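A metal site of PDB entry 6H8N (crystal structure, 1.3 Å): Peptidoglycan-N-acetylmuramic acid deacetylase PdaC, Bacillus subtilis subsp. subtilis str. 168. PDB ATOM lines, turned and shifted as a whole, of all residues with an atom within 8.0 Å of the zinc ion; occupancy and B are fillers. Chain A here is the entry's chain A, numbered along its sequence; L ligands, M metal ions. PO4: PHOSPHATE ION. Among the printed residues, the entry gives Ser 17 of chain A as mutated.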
ATOM      1  N   PHE A  16      -5.237  -6.039  31.829  1.00  0.00           N
ATOM      2  CA  PHE A  16      -4.370  -4.971  31.361  1.00  0.00           C
ATOM      3  C   PHE A  16      -3.233  -5.546  30.539  1.00  0.00           C
ATOM      4  O   PHE A  16      -2.442  -6.321  31.072  1.00  0.00           O
ATOM      5  CB  PHE A  16      -3.794  -4.183  32.534  1.00  0.00           C
ATOM      6  CG  PHE A  16      -4.850  -3.520  33.343  1.00  0.00           C
ATOM      7  CD1 PHE A  16      -5.369  -2.313  32.927  1.00  0.00           C
ATOM      8  CD2 PHE A  16      -5.330  -4.076  34.506  1.00  0.00           C
ATOM      9  CE1 PHE A  16      -6.343  -1.686  33.631  1.00  0.00           C
ATOM     10  CE2 PHE A  16      -6.329  -3.470  35.227  1.00  0.00           C
ATOM     11  CZ  PHE A  16      -6.849  -2.257  34.787  1.00  0.00           C
ATOM     12  N   SER A  17      -3.108  -5.110  29.299  1.00  0.00           N
ATOM     13  CA  SER A  17      -2.049  -5.571  28.404  1.00  0.00           C
ATOM     14  C   SER A  17      -1.044  -4.472  28.133  1.00  0.00           C
ATOM     15  O   SER A  17      -1.419  -3.302  28.003  1.00  0.00           O
ATOM     16  CB  SER A  17      -2.648  -5.968  27.065  1.00  0.00           C
ATOM     17  OG  SER A  17      -3.415  -7.153  27.181  1.00  0.00           O
ATOM     18  N   ASP A  18       0.216  -4.859  28.000  1.00  0.00           N
ATOM     19  CA  ASP A  18       1.313  -4.103  27.368  1.00  0.00           C
ATOM     20  C   ASP A  18       2.289  -3.500  28.343  1.00  0.00           C
ATOM     21  O   ASP A  18       3.334  -3.006  27.914  1.00  0.00           O
ATOM     22  CB  ASP A  18       0.856  -3.004  26.400  1.00  0.00           C
ATOM     23  CG  ASP A  18       0.136  -3.537  25.208  1.00  0.00           C
ATOM     24  OD1 ASP A  18       0.205  -4.741  24.955  1.00  0.00           O
ATOM     25  OD2 ASP A  18      -0.557  -2.718  24.545  1.00  0.00           O
ATOM     26  N   GLY A  19       2.018  -3.569  29.634  1.00  0.00           N
ATOM     27  CA  GLY A  19       2.949  -3.088  30.645  1.00  0.00           C
ATOM     28  C   GLY A  19       3.974  -4.170  30.977  1.00  0.00           C
ATOM     29  O   GLY A  19       4.052  -5.205  30.308  1.00  0.00           O
ATOM     30  N   PHE A  42      -1.217  -8.694  31.604  1.00  0.00           N
ATOM     31  CA  PHE A  42      -0.569  -9.446  30.534  1.00  0.00           C
ATOM     32  C   PHE A  42       0.616  -8.614  30.093  1.00  0.00           C
ATOM     33  O   PHE A  42       0.473  -7.582  29.432  1.00  0.00           O
ATOM     34  CB  PHE A  42      -1.582  -9.736  29.427  1.00  0.00           C
ATOM     35  CG  PHE A  42      -2.605 -10.747  29.840  1.00  0.00           C
ATOM     36  CD1 PHE A  42      -2.338 -12.087  29.693  1.00  0.00           C
ATOM     37  CD2 PHE A  42      -3.801 -10.362  30.432  1.00  0.00           C
ATOM     38  CE1 PHE A  42      -3.259 -13.045  30.111  1.00  0.00           C
ATOM     39  CE2 PHE A  42      -4.731 -11.311  30.853  1.00  0.00           C
ATOM     40  CZ  PHE A  42      -4.452 -12.655  30.666  1.00  0.00           C
ATOM     41  N   VAL A  43       1.797  -9.071  30.486  1.00  0.00           N
ATOM     42  CA  VAL A  43       3.011  -8.262  30.458  1.00  0.00           C
ATOM     43  C   VAL A  43       3.892  -8.659  29.278  1.00  0.00           C
ATOM     44  O   VAL A  43       3.948  -9.826  28.853  1.00  0.00           O
ATOM     45  CB  VAL A  43       3.808  -8.372  31.791  1.00  0.00           C
ATOM     46  CG1 VAL A  43       2.968  -7.862  32.950  1.00  0.00           C
ATOM     47  CG2 VAL A  43       4.288  -9.778  32.037  1.00  0.00           C
ATOM     48  N   LEU A  44       4.604  -7.665  28.769  1.00  0.00           N
ATOM     49  CA  LEU A  44       5.634  -7.850  27.755  1.00  0.00           C
ATOM     50  C   LEU A  44       6.949  -8.205  28.426  1.00  0.00           C
ATOM     51  O   LEU A  44       7.382  -7.506  29.348  1.00  0.00           O
ATOM     52  CB  LEU A  44       5.806  -6.571  26.937  1.00  0.00           C
ATOM     53  CG  LEU A  44       4.703  -6.363  25.908  1.00  0.00           C
ATOM     54  CD1 LEU A  44       4.798  -4.958  25.336  1.00  0.00           C
ATOM     55  CD2 LEU A  44       4.780  -7.359  24.774  1.00  0.00           C
ATOM     56  N   HIS A  68       2.401 -11.905  27.557  1.00  0.00           N
ATOM     57  CA  HIS A  68       1.926 -11.171  26.382  1.00  0.00           C
ATOM     58  C   HIS A  68       2.989 -11.078  25.299  1.00  0.00           C
ATOM     59  O   HIS A  68       2.938 -10.170  24.463  1.00  0.00           O
ATOM     60  CB  HIS A  68       1.435  -9.787  26.812  1.00  0.00           C
ATOM     61  CG  HIS A  68       0.585  -9.071  25.804  1.00  0.00           C
ATOM     62  ND1 HIS A  68      -0.439  -9.653  25.103  1.00  0.00           N
ATOM     63  CD2 HIS A  68       0.597  -7.757  25.454  1.00  0.00           C
ATOM     64  CE1 HIS A  68      -1.015  -8.734  24.324  1.00  0.00           C
ATOM     65  NE2 HIS A  68      -0.424  -7.576  24.535  1.00  0.00           N
ATOM     66  N   SER A  69       3.930 -12.031  25.294  1.00  0.00           N
ATOM     67  CA  SER A  69       5.070 -12.071  24.367  1.00  0.00           C
ATOM     68  C   SER A  69       6.201 -11.175  24.826  1.00  0.00           C
ATOM     69  O   SER A  69       6.074 -10.438  25.807  1.00  0.00           O
ATOM     70  CB  SER A  69       4.687 -11.740  22.912  1.00  0.00           C
ATOM     71  OG  SER A  69       4.734 -10.351  22.632  1.00  0.00           O
ATOM     72  N   HIS A  72       5.916  -8.054  21.314  1.00  0.00           N
ATOM     73  CA  HIS A  72       4.607  -7.717  20.736  1.00  0.00           C
ATOM     74  C   HIS A  72       4.509  -7.930  19.223  1.00  0.00           C
ATOM     75  O   HIS A  72       3.742  -7.207  18.583  1.00  0.00           O
ATOM     76  CB  HIS A  72       4.212  -6.256  21.054  1.00  0.00           C
ATOM     77  CG  HIS A  72       2.737  -6.072  21.282  1.00  0.00           C
ATOM     78  ND1 HIS A  72       1.830  -5.934  20.254  1.00  0.00           N
ATOM     79  CD2 HIS A  72       2.011  -5.998  22.431  1.00  0.00           C
ATOM     80  CE1 HIS A  72       0.606  -5.819  20.752  1.00  0.00           C
ATOM     81  NE2 HIS A  72       0.701  -5.844  22.072  1.00  0.00           N
ATOM     82  N   ARG A 106      -1.677 -14.374  26.399  1.00  0.00           N
ATOM     83  CA  ARG A 106      -2.540 -13.522  25.590  1.00  0.00           C
ATOM     84  C   ARG A 106      -1.756 -13.136  24.345  1.00  0.00           C
ATOM     85  O   ARG A 106      -0.895 -12.242  24.407  1.00  0.00           O
ATOM     86  CB  ARG A 106      -2.993 -12.309  26.376  1.00  0.00           C
ATOM     87  CG  ARG A 106      -3.869 -11.364  25.591  1.00  0.00           C
ATOM     88  CD  ARG A 106      -4.439 -10.291  26.489  1.00  0.00           C
ATOM     89  NE  ARG A 106      -5.595 -10.743  27.243  1.00  0.00           N
ATOM     90  CZ  ARG A 106      -6.276  -9.964  28.084  1.00  0.00           C
ATOM     91  NH1 ARG A 106      -5.887  -8.714  28.304  1.00  0.00           N
ATOM     92  NH2 ARG A 106      -7.354 -10.437  28.687  1.00  0.00           N
ATOM     93  N   PRO A 107      -1.985 -13.790  23.215  1.00  0.00           N
ATOM     94  CA  PRO A 107      -1.215 -13.482  22.004  1.00  0.00           C
ATOM     95  C   PRO A 107      -1.487 -12.060  21.553  1.00  0.00           C
ATOM     96  O   PRO A 107      -2.652 -11.644  21.526  1.00  0.00           O
ATOM     97  CB  PRO A 107      -1.753 -14.489  20.990  1.00  0.00           C
ATOM     98  CG  PRO A 107      -2.192 -15.663  21.826  1.00  0.00           C
ATOM     99  CD  PRO A 107      -2.812 -14.999  23.047  1.00  0.00           C
ATOM    100  N   PRO A 108      -0.455 -11.297  21.183  1.00  0.00           N
ATOM    101  CA  PRO A 108      -0.668  -9.938  20.668  1.00  0.00           C
ATOM    102  C   PRO A 108      -1.710  -9.905  19.571  1.00  0.00           C
ATOM    103  O   PRO A 108      -1.730 -10.759  18.668  1.00  0.00           O
ATOM    104  CB  PRO A 108       0.715  -9.563  20.140  1.00  0.00           C
ATOM    105  CG  PRO A 108       1.640 -10.277  21.097  1.00  0.00           C
ATOM    106  CD  PRO A 108       0.985 -11.599  21.307  1.00  0.00           C
ATOM    107  N   TYR A 109      -2.572  -8.886  19.624  1.00  0.00           N
ATOM    108  CA  TYR A 109      -3.637  -8.636  18.648  1.00  0.00           C
ATOM    109  C   TYR A 109      -4.673  -9.753  18.583  1.00  0.00           C
ATOM    110  O   TYR A 109      -5.518  -9.743  17.685  1.00  0.00           O
ATOM    111  CB  TYR A 109      -3.098  -8.330  17.238  1.00  0.00           C
ATOM    112  CG  TYR A 109      -1.894  -7.416  17.241  1.00  0.00           C
ATOM    113  CD1 TYR A 109      -2.023  -6.063  17.519  1.00  0.00           C
ATOM    114  CD2 TYR A 109      -0.622  -7.908  16.996  1.00  0.00           C
ATOM    115  CE1 TYR A 109      -0.940  -5.231  17.545  1.00  0.00           C
ATOM    116  CE2 TYR A 109       0.466  -7.087  17.009  1.00  0.00           C
ATOM    117  CZ  TYR A 109       0.316  -5.747  17.290  1.00  0.00           C
ATOM    118  OH  TYR A 109       1.404  -4.912  17.324  1.00  0.00           O
ATOM    119  N   GLY A 110      -4.647 -10.700  19.520  1.00  0.00           N
ATOM    120  CA  GLY A 110      -5.501 -11.873  19.496  1.00  0.00           C
ATOM    121  C   GLY A 110      -5.084 -12.934  18.504  1.00  0.00           C
ATOM    122  O   GLY A 110      -5.798 -13.927  18.350  1.00  0.00           O
ATOM    123  N   TRP A 127     -10.609 -11.729  25.652  1.00  0.00           N
ATOM    124  CA  TRP A 127     -11.431 -10.723  26.329  1.00  0.00           C
ATOM    125  C   TRP A 127     -12.791 -10.620  25.640  1.00  0.00           C
ATOM    126  O   TRP A 127     -12.975 -11.094  24.520  1.00  0.00           O
ATOM    127  CB  TRP A 127     -10.738  -9.360  26.321  1.00  0.00           C
ATOM    128  CG  TRP A 127     -10.433  -8.911  24.950  1.00  0.00           C
ATOM    129  CD1 TRP A 127     -11.273  -8.244  24.107  1.00  0.00           C
ATOM    130  CD2 TRP A 127      -9.231  -9.143  24.211  1.00  0.00           C
ATOM    131  NE1 TRP A 127     -10.667  -8.045  22.900  1.00  0.00           N
ATOM    132  CE2 TRP A 127      -9.407  -8.593  22.925  1.00  0.00           C
ATOM    133  CE3 TRP A 127      -8.005  -9.760  24.507  1.00  0.00           C
ATOM    134  CZ2 TRP A 127      -8.412  -8.647  21.939  1.00  0.00           C
ATOM    135  CZ3 TRP A 127      -7.033  -9.803  23.544  1.00  0.00           C
ATOM    136  CH2 TRP A 127      -7.236  -9.245  22.270  1.00  0.00           C
ATOM    137  N   LEU A 157     -10.636  -5.492  28.438  1.00  0.00           N
ATOM    138  CA  LEU A 157      -9.274  -5.189  27.993  1.00  0.00           C
ATOM    139  C   LEU A 157      -8.988  -3.698  28.061  1.00  0.00           C
ATOM    140  O   LEU A 157      -9.651  -2.907  27.387  1.00  0.00           O
ATOM    141  CB  LEU A 157      -9.065  -5.682  26.567  1.00  0.00           C
ATOM    142  CG  LEU A 157      -7.790  -5.244  25.844  1.00  0.00           C
ATOM    143  CD1 LEU A 157      -6.558  -5.727  26.605  1.00  0.00           C
ATOM    144  CD2 LEU A 157      -7.793  -5.732  24.402  1.00  0.00           C
ATOM    145  N   ILE A 158      -7.972  -3.319  28.840  1.00  0.00           N
ATOM    146  CA  ILE A 158      -7.402  -1.976  28.854  1.00  0.00           C
ATOM    147  C   ILE A 158      -5.904  -2.126  28.631  1.00  0.00           C
ATOM    148  O   ILE A 158      -5.304  -3.131  29.046  1.00  0.00           O
ATOM    149  CB  ILE A 158      -7.700  -1.299  30.212  1.00  0.00           C
ATOM    150  CG1 ILE A 158      -9.215  -1.128  30.383  1.00  0.00           C
ATOM    151  CG2 ILE A 158      -6.947   0.023  30.375  1.00  0.00           C
ATOM    152  CD1 ILE A 158      -9.656  -0.708  31.751  1.00  0.00           C
ATOM    153  N   HIS A 159      -5.271  -1.161  27.974  1.00  0.00           N
ATOM    154  CA  HIS A 159      -3.825  -1.205  27.747  1.00  0.00           C
ATOM    155  C   HIS A 159      -3.160  -0.258  28.739  1.00  0.00           C
ATOM    156  O   HIS A 159      -3.344   0.958  28.649  1.00  0.00           O
ATOM    157  CB  HIS A 159      -3.516  -0.869  26.292  1.00  0.00           C
ATOM    158  CG  HIS A 159      -4.186  -1.802  25.333  1.00  0.00           C
ATOM    159  ND1 HIS A 159      -5.480  -1.619  24.880  1.00  0.00           N
ATOM    160  CD2 HIS A 159      -3.778  -2.985  24.806  1.00  0.00           C
ATOM    161  CE1 HIS A 159      -5.818  -2.624  24.093  1.00  0.00           C
ATOM    162  NE2 HIS A 159      -4.808  -3.475  24.033  1.00  0.00           N
ATOM    163  N   ILE A 161      -0.505   1.344  29.358  1.00  0.00           N
ATOM    164  CA  ILE A 161       0.655   2.117  28.953  1.00  0.00           C
ATOM    165  C   ILE A 161       0.308   3.566  28.617  1.00  0.00           C
ATOM    166  O   ILE A 161       1.206   4.326  28.249  1.00  0.00           O
ATOM    167  CB  ILE A 161       1.396   1.433  27.787  1.00  0.00           C
ATOM    168  CG1 ILE A 161       0.486   1.252  26.581  1.00  0.00           C
ATOM    169  CG2 ILE A 161       1.944   0.096  28.270  1.00  0.00           C
ATOM    170  CD1 ILE A 161       1.232   0.871  25.320  1.00  0.00           C
HETATM  171  P   PO4 L   1      -3.279  -5.826  22.060  1.00  0.00           P
HETATM  172  O1  PO4 L   1      -3.290  -4.965  20.764  1.00  0.00           O
HETATM  173  O2  PO4 L   1      -4.669  -5.777  22.647  1.00  0.00           O
HETATM  174  O3  PO4 L   1      -2.358  -5.129  23.023  1.00  0.00           O
HETATM  175  O4  PO4 L   1      -2.781  -7.196  21.727  1.00  0.00           O
HETATM  176 ZN    ZN M   1      -0.661  -5.784  23.560  1.00  0.00          ZN
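The backbone NH of His 72 lies within hydrogen-bond range of the side-chain hydroxyl of Ser 69 (2.9 Å).
ND1 of His 72 lies within hydrogen-bond range of OH of Tyr 109 (3.1 Å).
The backbone NH of His 68 lies within hydrogen-bond range of the backbone carbonyl oxygen of Val 43 (2.9 Å).
A ring nitrogen (ND1) of His 68 sits at hydrogen-bond distance from the backbone carbonyl oxygen (O) of Arg 106 (2.7 Å).
N of Asp 18 is in hydrogen-bond range of O of Phe 42 (3.1 Å).
Three residues have an atom within 4 Å of the zinc ion: Asp 18, His 68 and His 72.
The nearest printed residue that does not touch the zinc ion is Ser 17 (4.03 Å).
The zinc ion is bound by O3 of the ligand (1.9 Å).
OD1 of Asp 18 is bound to the zinc ion (1.9 Å).
The zinc ion is bound by NE2 of His 72 (2.0 Å).
NE2 of His 68 binds the zinc ion (2.1 Å).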
